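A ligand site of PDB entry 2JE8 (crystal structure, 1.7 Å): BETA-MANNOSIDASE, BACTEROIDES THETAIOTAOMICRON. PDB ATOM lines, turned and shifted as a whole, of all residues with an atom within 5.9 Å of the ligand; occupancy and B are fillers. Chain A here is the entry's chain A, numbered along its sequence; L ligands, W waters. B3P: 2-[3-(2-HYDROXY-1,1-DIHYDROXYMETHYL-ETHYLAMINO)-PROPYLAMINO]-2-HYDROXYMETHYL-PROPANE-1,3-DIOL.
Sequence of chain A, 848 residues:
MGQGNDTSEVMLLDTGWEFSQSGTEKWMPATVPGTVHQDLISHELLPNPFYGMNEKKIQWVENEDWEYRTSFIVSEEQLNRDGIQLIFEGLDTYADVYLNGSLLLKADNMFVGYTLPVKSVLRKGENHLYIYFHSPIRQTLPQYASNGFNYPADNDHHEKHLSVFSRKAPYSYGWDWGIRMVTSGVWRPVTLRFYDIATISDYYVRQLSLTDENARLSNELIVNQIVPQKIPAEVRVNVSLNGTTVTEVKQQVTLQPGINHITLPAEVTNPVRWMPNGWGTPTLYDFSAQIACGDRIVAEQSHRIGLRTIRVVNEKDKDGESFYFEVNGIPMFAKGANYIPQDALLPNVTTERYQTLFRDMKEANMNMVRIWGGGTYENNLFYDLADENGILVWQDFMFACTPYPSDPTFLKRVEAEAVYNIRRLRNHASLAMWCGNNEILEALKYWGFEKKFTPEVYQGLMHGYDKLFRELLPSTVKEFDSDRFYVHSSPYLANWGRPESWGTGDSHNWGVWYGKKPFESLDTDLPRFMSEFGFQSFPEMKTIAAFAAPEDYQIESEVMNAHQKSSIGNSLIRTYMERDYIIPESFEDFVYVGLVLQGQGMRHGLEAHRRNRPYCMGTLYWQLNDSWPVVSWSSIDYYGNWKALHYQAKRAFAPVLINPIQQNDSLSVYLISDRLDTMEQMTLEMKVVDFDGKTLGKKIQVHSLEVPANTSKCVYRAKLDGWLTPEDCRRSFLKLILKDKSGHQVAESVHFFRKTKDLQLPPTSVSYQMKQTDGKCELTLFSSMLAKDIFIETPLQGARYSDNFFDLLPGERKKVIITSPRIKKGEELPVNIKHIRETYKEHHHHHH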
ATOM      1  N   ASN A 155     -14.780  16.658   4.296  1.00  0.00           N
ATOM      2  CA  ASN A 155     -16.207  16.350   4.363  1.00  0.00           C
ATOM      3  C   ASN A 155     -16.904  16.161   3.021  1.00  0.00           C
ATOM      4  O   ASN A 155     -18.056  15.751   2.972  1.00  0.00           O
ATOM      5  CB  ASN A 155     -16.965  17.364   5.231  1.00  0.00           C
ATOM      6  CG  ASN A 155     -16.688  17.139   6.701  1.00  0.00           C
ATOM      7  OD1 ASN A 155     -17.158  16.157   7.298  1.00  0.00           O
ATOM      8  ND2 ASN A 155     -15.862  18.017   7.288  1.00  0.00           N
ATOM      9  N   TRP A 175     -20.924  14.446   4.880  1.00  0.00           N
ATOM     10  CA  TRP A 175     -20.372  15.138   6.036  1.00  0.00           C
ATOM     11  C   TRP A 175     -19.997  14.083   7.076  1.00  0.00           C
ATOM     12  O   TRP A 175     -20.316  12.898   6.904  1.00  0.00           O
ATOM     13  CB  TRP A 175     -21.335  16.215   6.620  1.00  0.00           C
ATOM     14  CG  TRP A 175     -20.556  17.376   7.204  1.00  0.00           C
ATOM     15  CD1 TRP A 175     -20.137  17.497   8.510  1.00  0.00           C
ATOM     16  CD2 TRP A 175     -20.031  18.485   6.497  1.00  0.00           C
ATOM     17  NE1 TRP A 175     -19.391  18.653   8.659  1.00  0.00           N
ATOM     18  CE2 TRP A 175     -19.315  19.285   7.444  1.00  0.00           C
ATOM     19  CE3 TRP A 175     -20.109  18.913   5.159  1.00  0.00           C
ATOM     20  CZ2 TRP A 175     -18.678  20.501   7.086  1.00  0.00           C
ATOM     21  CZ3 TRP A 175     -19.457  20.096   4.794  1.00  0.00           C
ATOM     22  CH2 TRP A 175     -18.747  20.880   5.758  1.00  0.00           C
ATOM     23  N   ASP A 176     -19.442  14.537   8.197  1.00  0.00           N
ATOM     24  CA  ASP A 176     -18.945  13.590   9.225  1.00  0.00           C
ATOM     25  C   ASP A 176     -20.093  13.017  10.077  1.00  0.00           C
ATOM     26  O   ASP A 176     -19.840  12.190  10.955  1.00  0.00           O
ATOM     27  CB  ASP A 176     -17.763  14.207  10.044  1.00  0.00           C
ATOM     28  CG  ASP A 176     -18.155  15.409  10.901  1.00  0.00           C
ATOM     29  OD1 ASP A 176     -19.374  15.717  11.064  1.00  0.00           O
ATOM     30  OD2 ASP A 176     -17.240  16.012  11.474  1.00  0.00           O
ATOM     31  N   TRP A 177     -21.343  13.408   9.748  1.00  0.00           N
ATOM     32  CA  TRP A 177     -22.565  12.784  10.252  1.00  0.00           C
ATOM     33  C   TRP A 177     -23.547  12.428   9.142  1.00  0.00           C
ATOM     34  O   TRP A 177     -24.683  12.073   9.435  1.00  0.00           O
ATOM     35  CB  TRP A 177     -23.286  13.731  11.250  1.00  0.00           C
ATOM     36  CG  TRP A 177     -23.325  15.186  10.756  1.00  0.00           C
ATOM     37  CD1 TRP A 177     -22.511  16.207  11.172  1.00  0.00           C
ATOM     38  CD2 TRP A 177     -24.139  15.734   9.695  1.00  0.00           C
ATOM     39  NE1 TRP A 177     -22.780  17.356  10.464  1.00  0.00           N
ATOM     40  CE2 TRP A 177     -23.778  17.108   9.569  1.00  0.00           C
ATOM     41  CE3 TRP A 177     -25.180  15.222   8.892  1.00  0.00           C
ATOM     42  CZ2 TRP A 177     -24.421  17.983   8.670  1.00  0.00           C
ATOM     43  CZ3 TRP A 177     -25.808  16.098   7.953  1.00  0.00           C
ATOM     44  CH2 TRP A 177     -25.396  17.457   7.837  1.00  0.00           C
ATOM     45  N   ARG A 370     -27.809  27.168  17.220  1.00  0.00           N
ATOM     46  CA  ARG A 370     -26.863  27.592  16.182  1.00  0.00           C
ATOM     47  C   ARG A 370     -27.256  26.889  14.877  1.00  0.00           C
ATOM     48  O   ARG A 370     -27.246  25.634  14.764  1.00  0.00           O
ATOM     49  CB  ARG A 370     -25.420  27.256  16.606  1.00  0.00           C
ATOM     50  CG  ARG A 370     -24.421  27.478  15.465  1.00  0.00           C
ATOM     51  CD  ARG A 370     -22.981  27.553  15.986  1.00  0.00           C
ATOM     52  NE  ARG A 370     -22.029  27.570  14.867  1.00  0.00           N
ATOM     53  CZ  ARG A 370     -20.998  26.726  14.729  1.00  0.00           C
ATOM     54  NH1 ARG A 370     -20.817  25.709  15.602  1.00  0.00           N
ATOM     55  NH2 ARG A 370     -20.160  26.885  13.706  1.00  0.00           N
ATOM     56  N   TRP A 372     -25.793  25.898  11.935  1.00  0.00           N
ATOM     57  CA  TRP A 372     -24.375  25.672  11.610  1.00  0.00           C
ATOM     58  C   TRP A 372     -24.089  25.731  10.090  1.00  0.00           C
ATOM     59  O   TRP A 372     -24.938  25.346   9.243  1.00  0.00           O
ATOM     60  CB  TRP A 372     -23.997  24.346  12.263  1.00  0.00           C
ATOM     61  CG  TRP A 372     -22.772  23.644  11.780  1.00  0.00           C
ATOM     62  CD1 TRP A 372     -21.505  23.677  12.338  1.00  0.00           C
ATOM     63  CD2 TRP A 372     -22.732  22.707  10.708  1.00  0.00           C
ATOM     64  NE1 TRP A 372     -20.681  22.822  11.617  1.00  0.00           N
ATOM     65  CE2 TRP A 372     -21.416  22.190  10.639  1.00  0.00           C
ATOM     66  CE3 TRP A 372     -23.733  22.183   9.856  1.00  0.00           C
ATOM     67  CZ2 TRP A 372     -21.055  21.244   9.698  1.00  0.00           C
ATOM     68  CZ3 TRP A 372     -23.380  21.261   8.886  1.00  0.00           C
ATOM     69  CH2 TRP A 372     -22.043  20.778   8.829  1.00  0.00           C
ATOM     70  N   CYS A 401     -15.530  24.180   7.382  1.00  0.00           N
ATOM     71  CA  CYS A 401     -14.480  23.161   7.555  1.00  0.00           C
ATOM     72  C   CYS A 401     -13.333  23.253   6.564  1.00  0.00           C
ATOM     73  O   CYS A 401     -12.207  22.814   6.890  1.00  0.00           O
ATOM     74  CB  CYS A 401     -15.078  21.753   7.646  1.00  0.00           C
ATOM     75  SG  CYS A 401     -15.999  21.496   9.186  1.00  0.00           S
ATOM     76  N   ASN A 438     -17.935  28.006   9.974  1.00  0.00           N
ATOM     77  CA  ASN A 438     -17.550  26.988  10.966  1.00  0.00           C
ATOM     78  C   ASN A 438     -16.103  26.497  10.722  1.00  0.00           C
ATOM     79  O   ASN A 438     -15.847  25.859   9.687  1.00  0.00           O
ATOM     80  CB  ASN A 438     -18.463  25.777  10.855  1.00  0.00           C
ATOM     81  CG  ASN A 438     -18.076  24.702  11.823  1.00  0.00           C
ATOM     82  OD1 ASN A 438     -18.325  24.845  13.043  1.00  0.00           O
ATOM     83  ND2 ASN A 438     -17.416  23.625  11.326  1.00  0.00           N
ATOM     84  N   GLU A 439     -15.216  26.798  11.684  1.00  0.00           N
ATOM     85  CA  GLU A 439     -13.904  26.128  11.823  1.00  0.00           C
ATOM     86  C   GLU A 439     -12.895  26.330  10.672  1.00  0.00           C
ATOM     87  O   GLU A 439     -11.886  25.584  10.576  1.00  0.00           O
ATOM     88  CB  GLU A 439     -14.070  24.604  12.094  1.00  0.00           C
ATOM     89  CG  GLU A 439     -14.655  24.350  13.521  1.00  0.00           C
ATOM     90  CD  GLU A 439     -15.039  22.884  13.790  1.00  0.00           C
ATOM     91  OE1 GLU A 439     -15.265  22.084  12.824  1.00  0.00           O
ATOM     92  OE2 GLU A 439     -15.221  22.568  14.978  1.00  0.00           O
ATOM     93  N   GLU A 442      -9.541  27.725  12.043  1.00  0.00           N
ATOM     94  CA  GLU A 442      -8.944  26.557  12.731  1.00  0.00           C
ATOM     95  C   GLU A 442      -8.261  25.580  11.749  1.00  0.00           C
ATOM     96  O   GLU A 442      -7.095  25.166  11.957  1.00  0.00           O
ATOM     97  CB  GLU A 442      -9.993  25.839  13.566  1.00  0.00           C
ATOM     98  CG  GLU A 442      -9.456  24.485  14.118  1.00  0.00           C
ATOM     99  CD  GLU A 442     -10.313  23.930  15.222  1.00  0.00           C
ATOM    100  OE1 GLU A 442     -10.470  24.584  16.273  1.00  0.00           O
ATOM    101  OE2 GLU A 442     -10.751  22.781  15.081  1.00  0.00           O
ATOM    102  N   TRP A 447      -4.187  22.431  10.733  1.00  0.00           N
ATOM    103  CA  TRP A 447      -4.118  21.175   9.975  1.00  0.00           C
ATOM    104  C   TRP A 447      -2.852  21.093   9.090  1.00  0.00           C
ATOM    105  O   TRP A 447      -2.753  20.210   8.216  1.00  0.00           O
ATOM    106  CB  TRP A 447      -5.348  21.013   9.099  1.00  0.00           C
ATOM    107  CG  TRP A 447      -6.716  20.923   9.806  1.00  0.00           C
ATOM    108  CD1 TRP A 447      -7.007  21.202  11.123  1.00  0.00           C
ATOM    109  CD2 TRP A 447      -7.951  20.577   9.194  1.00  0.00           C
ATOM    110  NE1 TRP A 447      -8.359  21.031  11.365  1.00  0.00           N
ATOM    111  CE2 TRP A 447      -8.966  20.640  10.192  1.00  0.00           C
ATOM    112  CE3 TRP A 447      -8.312  20.207   7.881  1.00  0.00           C
ATOM    113  CZ2 TRP A 447     -10.311  20.345   9.915  1.00  0.00           C
ATOM    114  CZ3 TRP A 447      -9.656  19.907   7.618  1.00  0.00           C
ATOM    115  CH2 TRP A 447     -10.635  19.989   8.633  1.00  0.00           C
ATOM    116  N   TRP A 496      -8.899  23.401  20.710  1.00  0.00           N
ATOM    117  CA  TRP A 496      -9.069  22.408  21.778  1.00  0.00           C
ATOM    118  C   TRP A 496      -7.722  21.783  22.184  1.00  0.00           C
ATOM    119  O   TRP A 496      -7.632  21.151  23.246  1.00  0.00           O
ATOM    120  CB  TRP A 496     -10.099  21.349  21.444  1.00  0.00           C
ATOM    121  CG  TRP A 496      -9.872  20.400  20.296  1.00  0.00           C
ATOM    122  CD1 TRP A 496     -10.297  20.542  18.990  1.00  0.00           C
ATOM    123  CD2 TRP A 496      -9.265  19.083  20.385  1.00  0.00           C
ATOM    124  NE1 TRP A 496      -9.963  19.385  18.251  1.00  0.00           N
ATOM    125  CE2 TRP A 496      -9.320  18.502  19.085  1.00  0.00           C
ATOM    126  CE3 TRP A 496      -8.631  18.379  21.416  1.00  0.00           C
ATOM    127  CZ2 TRP A 496      -8.794  17.222  18.801  1.00  0.00           C
ATOM    128  CZ3 TRP A 496      -8.099  17.071  21.143  1.00  0.00           C
ATOM    129  CH2 TRP A 496      -8.185  16.530  19.839  1.00  0.00           C
ATOM    130  N   HIS A 508     -14.797  25.319  20.554  1.00  0.00           N
ATOM    131  CA  HIS A 508     -15.267  23.982  20.119  1.00  0.00           C
ATOM    132  C   HIS A 508     -14.308  23.009  20.806  1.00  0.00           C
ATOM    133  O   HIS A 508     -13.274  22.636  20.219  1.00  0.00           O
ATOM    134  CB  HIS A 508     -15.155  23.797  18.594  1.00  0.00           C
ATOM    135  CG  HIS A 508     -16.070  24.698  17.811  1.00  0.00           C
ATOM    136  ND1 HIS A 508     -16.417  24.436  16.493  1.00  0.00           N
ATOM    137  CD2 HIS A 508     -16.686  25.850  18.140  1.00  0.00           C
ATOM    138  CE1 HIS A 508     -17.183  25.420  16.045  1.00  0.00           C
ATOM    139  NE2 HIS A 508     -17.383  26.272  17.028  1.00  0.00           N
ATOM    140  N   TRP A 510     -13.180  19.799  21.502  1.00  0.00           N
ATOM    141  CA  TRP A 510     -13.343  18.417  21.038  1.00  0.00           C
ATOM    142  C   TRP A 510     -12.318  17.445  21.686  1.00  0.00           C
ATOM    143  O   TRP A 510     -12.048  16.364  21.132  1.00  0.00           O
ATOM    144  CB  TRP A 510     -13.296  18.363  19.491  1.00  0.00           C
ATOM    145  CG  TRP A 510     -14.629  18.781  18.900  1.00  0.00           C
ATOM    146  CD1 TRP A 510     -14.938  20.006  18.303  1.00  0.00           C
ATOM    147  CD2 TRP A 510     -15.836  18.040  18.955  1.00  0.00           C
ATOM    148  NE1 TRP A 510     -16.285  20.024  17.976  1.00  0.00           N
ATOM    149  CE2 TRP A 510     -16.850  18.833  18.342  1.00  0.00           C
ATOM    150  CE3 TRP A 510     -16.159  16.738  19.420  1.00  0.00           C
ATOM    151  CZ2 TRP A 510     -18.165  18.363  18.167  1.00  0.00           C
ATOM    152  CZ3 TRP A 510     -17.480  16.289  19.309  1.00  0.00           C
ATOM    153  CH2 TRP A 510     -18.462  17.089  18.632  1.00  0.00           C
ATOM    154  N   TYR A 514     -13.020  13.489  19.940  1.00  0.00           N
ATOM    155  CA  TYR A 514     -11.827  13.479  19.078  1.00  0.00           C
ATOM    156  C   TYR A 514     -10.509  13.325  19.816  1.00  0.00           C
ATOM    157  O   TYR A 514      -9.590  12.639  19.318  1.00  0.00           O
ATOM    158  CB  TYR A 514     -11.787  14.735  18.195  1.00  0.00           C
ATOM    159  CG  TYR A 514     -12.856  14.689  17.121  1.00  0.00           C
ATOM    160  CD1 TYR A 514     -12.831  13.708  16.118  1.00  0.00           C
ATOM    161  CD2 TYR A 514     -13.935  15.597  17.146  1.00  0.00           C
ATOM    162  CE1 TYR A 514     -13.819  13.685  15.112  1.00  0.00           C
ATOM    163  CE2 TYR A 514     -14.915  15.581  16.173  1.00  0.00           C
ATOM    164  CZ  TYR A 514     -14.871  14.626  15.177  1.00  0.00           C
ATOM    165  OH  TYR A 514     -15.837  14.623  14.192  1.00  0.00           O
ATOM    166  N   GLU A 532     -19.325  24.380  20.651  1.00  0.00           N
ATOM    167  CA  GLU A 532     -19.469  22.949  20.280  1.00  0.00           C
ATOM    168  C   GLU A 532     -18.728  22.121  21.316  1.00  0.00           C
ATOM    169  O   GLU A 532     -17.600  22.449  21.688  1.00  0.00           O
ATOM    170  CB  GLU A 532     -18.788  22.599  18.928  1.00  0.00           C
ATOM    171  CG  GLU A 532     -19.479  23.117  17.701  1.00  0.00           C
ATOM    172  CD  GLU A 532     -18.884  22.563  16.393  1.00  0.00           C
ATOM    173  OE1 GLU A 532     -18.061  21.611  16.431  1.00  0.00           O
ATOM    174  OE2 GLU A 532     -19.265  23.095  15.330  1.00  0.00           O
ATOM    175  N   SER A 567     -14.234  10.726  11.608  1.00  0.00           N
ATOM    176  CA  SER A 567     -12.853  10.257  11.459  1.00  0.00           C
ATOM    177  C   SER A 567     -12.432   9.273  12.574  1.00  0.00           C
ATOM    178  O   SER A 567     -11.383   8.610  12.437  1.00  0.00           O
ATOM    179  CB  SER A 567     -11.920  11.467  11.444  1.00  0.00           C
ATOM    180  OG  SER A 567     -11.912  12.056  12.723  1.00  0.00           O
ATOM    181  N   TRP A 622     -22.936  19.819  20.416  1.00  0.00           N
ATOM    182  CA  TRP A 622     -22.927  19.258  19.054  1.00  0.00           C
ATOM    183  C   TRP A 622     -23.466  17.821  19.248  1.00  0.00           C
ATOM    184  O   TRP A 622     -22.770  17.026  19.873  1.00  0.00           O
ATOM    185  CB  TRP A 622     -21.475  19.220  18.499  1.00  0.00           C
ATOM    186  CG  TRP A 622     -21.564  18.707  17.123  1.00  0.00           C
ATOM    187  CD1 TRP A 622     -21.527  17.369  16.720  1.00  0.00           C
ATOM    188  CD2 TRP A 622     -21.889  19.476  15.947  1.00  0.00           C
ATOM    189  NE1 TRP A 622     -21.742  17.298  15.338  1.00  0.00           N
ATOM    190  CE2 TRP A 622     -22.022  18.569  14.864  1.00  0.00           C
ATOM    191  CE3 TRP A 622     -22.091  20.855  15.721  1.00  0.00           C
ATOM    192  CZ2 TRP A 622     -22.349  18.983  13.562  1.00  0.00           C
ATOM    193  CZ3 TRP A 622     -22.381  21.285  14.412  1.00  0.00           C
ATOM    194  CH2 TRP A 622     -22.526  20.334  13.337  1.00  0.00           C
ATOM    195  N   TRP A 633     -23.588  12.415  16.942  1.00  0.00           N
ATOM    196  CA  TRP A 633     -23.604  13.129  18.190  1.00  0.00           C
ATOM    197  C   TRP A 633     -25.007  13.661  18.591  1.00  0.00           C
ATOM    198  O   TRP A 633     -25.107  14.423  19.555  1.00  0.00           O
ATOM    199  CB  TRP A 633     -22.710  14.331  18.016  1.00  0.00           C
ATOM    200  CG  TRP A 633     -21.267  13.968  17.693  1.00  0.00           C
ATOM    201  CD1 TRP A 633     -20.254  13.754  18.593  1.00  0.00           C
ATOM    202  CD2 TRP A 633     -20.678  13.841  16.381  1.00  0.00           C
ATOM    203  NE1 TRP A 633     -19.063  13.519  17.925  1.00  0.00           N
ATOM    204  CE2 TRP A 633     -19.307  13.524  16.563  1.00  0.00           C
ATOM    205  CE3 TRP A 633     -21.181  13.962  15.061  1.00  0.00           C
ATOM    206  CZ2 TRP A 633     -18.404  13.378  15.501  1.00  0.00           C
ATOM    207  CZ3 TRP A 633     -20.288  13.770  13.982  1.00  0.00           C
ATOM    208  CH2 TRP A 633     -18.924  13.448  14.209  1.00  0.00           C
HETATM  209  C1  B3P L   1     -14.508  19.020  13.866  1.00  0.00           C
HETATM  210  C2  B3P L   1     -15.617  19.345  14.858  1.00  0.00           C
HETATM  211  C3  B3P L   1     -13.261  18.507  14.615  1.00  0.00           C
HETATM  212  N1  B3P L   1     -12.164  18.374  13.640  1.00  0.00           N
HETATM  213  C4  B3P L   1     -11.063  17.407  13.850  1.00  0.00           C
HETATM  214  C5  B3P L   1     -10.527  17.466  15.284  1.00  0.00           C
HETATM  215  C6  B3P L   1     -11.616  16.002  13.644  1.00  0.00           C
HETATM  216  C7  B3P L   1     -10.000  17.757  12.797  1.00  0.00           C
HETATM  217  N2  B3P L   1     -16.761  20.126  14.296  1.00  0.00           N
HETATM  218  C8  B3P L   1     -17.801  19.415  13.528  1.00  0.00           C
HETATM  219  C9  B3P L   1     -19.050  20.354  13.595  1.00  0.00           C
HETATM  220  C10 B3P L   1     -17.322  19.280  12.066  1.00  0.00           C
HETATM  221  C11 B3P L   1     -18.154  18.051  14.149  1.00  0.00           C
HETATM  222  O1  B3P L   1     -18.602  21.714  13.251  1.00  0.00           O
HETATM  223  O2  B3P L   1     -18.378  18.692  11.273  1.00  0.00           O
HETATM  224  O3  B3P L   1     -17.171  17.027  13.821  1.00  0.00           O
HETATM  225  O4  B3P L   1      -9.930  18.748  15.473  1.00  0.00           O
HETATM  226  O5  B3P L   1     -12.392  15.918  12.417  1.00  0.00           O
HETATM  227  O6  B3P L   1      -9.061  16.659  12.753  1.00  0.00           O
HETATM  228  O   HOH W   1     -13.201  18.399  10.779  1.00  0.00           O
HETATM  229  O   HOH W   2      -7.499  21.191  16.021  1.00  0.00           O
HETATM  230  O   HOH W   3     -10.132  14.188  11.237  1.00  0.00           O
HETATM  231  O   HOH W   4      -6.572  17.488  10.850  1.00  0.00           O
HETATM  232  O   HOH W   5     -10.960  21.086  12.855  1.00  0.00           O
HETATM  233  O   HOH W   6     -14.697  13.602  11.749  1.00  0.00           O
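An oxygen (O1) of the ligand lies within hydrogen-bond range of the side-chain amide nitrogen (ND2) of Asn 438 (3.0 Å). O3 of the ligand lies within hydrogen-bond range of OH of Tyr 514 (2.8 Å). The indole nitrogen (NE1) of Trp 496 sits at hydrogen-bond distance from an oxygen (O4) of the ligand, 2.9 Å away. NE1 of Trp 372 is in hydrogen-bond range of O1 of the ligand (2.9 Å). An oxygen (O2) of the ligand sits at hydrogen-bond distance from the indole nitrogen (NE1) of Trp 175 (2.8 Å). OE1 of Glu 532 is in salt-bridge range of N2 of the ligand. An oxygen (O3) of the ligand sits at hydrogen-bond distance from the side-chain carboxylate (OD2) of Asp 176. The side-chain carboxylate (OE1) of Glu 439 is in salt-bridge range of a nitrogen (N2) of the ligand (2.9 Å).
The side-chain carboxylate (OE1) of Glu 439 lies within hydrogen-bond range of the side-chain sulfur (SG) of Cys 401. The backbone carbonyl oxygen (O) of Asn 438 is in hydrogen-bond range of the backbone NH (N) of Cys 401 (2.9 Å). The backbone NH of Asp 176 is in hydrogen-bond range of the side-chain amide oxygen of Asn 155, 2.9 Å away. The guanidinium group (NH2) of Arg 370 is in hydrogen-bond range of the side-chain amide oxygen (OD1) of Asn 438, at 2.8 Å. OE2 of Glu 532 lies within salt-bridge range of NH1 of Arg 370, at 3.1 Å. The side-chain amide nitrogen (ND2) of Asn 438 sits close to the indole nitrogen (NE1) of Trp 372, 3.4 Å away. A ring nitrogen (ND1) of His 508 sits at hydrogen-bond distance from the side-chain carboxylate (OE2) of Glu 439, 2.7 Å away. OE1 of Glu 532 sits close to ND1 of His 508, at 3.3 Å.
Cys 401 touches the ligand. Trp 447 touches the ligand (CZ2 to C7, 3.9 Å). NE1 of Trp 510 touches C2 of the ligand, 3.3 Å away. Ser 567 touches the ligand (OG to O5, 3.9 Å). Trp 622 touches the ligand (CH2 to C9, 3.5 Å). Hydrophobic or aromatic side chains that line the ligand: Trp 175, Trp 372, Trp 447, Trp 496, Trp 510, Tyr 514 and Trp 622. 13 residues have an atom within 4 Å of the ligand: Trp 175, Asp 176, Trp 372, Cys 401, Asn 438, Glu 439, Trp 447, Trp 496, Trp 510, Tyr 514, Glu 532, Ser 567 and Trp 622.
Water W5 lies within hydrogen-bond range of OE2 of Glu 442 (2.8 Å), NE1 of Trp 447 (3.0 Å) and N1 of the ligand (3.1 Å). Water W3 bridges O5 of the ligand (3.1 Å) and OG of Ser 567 (3.1 Å). Water W6 lies within hydrogen-bond range of OH of Tyr 514, N of Ser 567 and O5 of the ligand.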
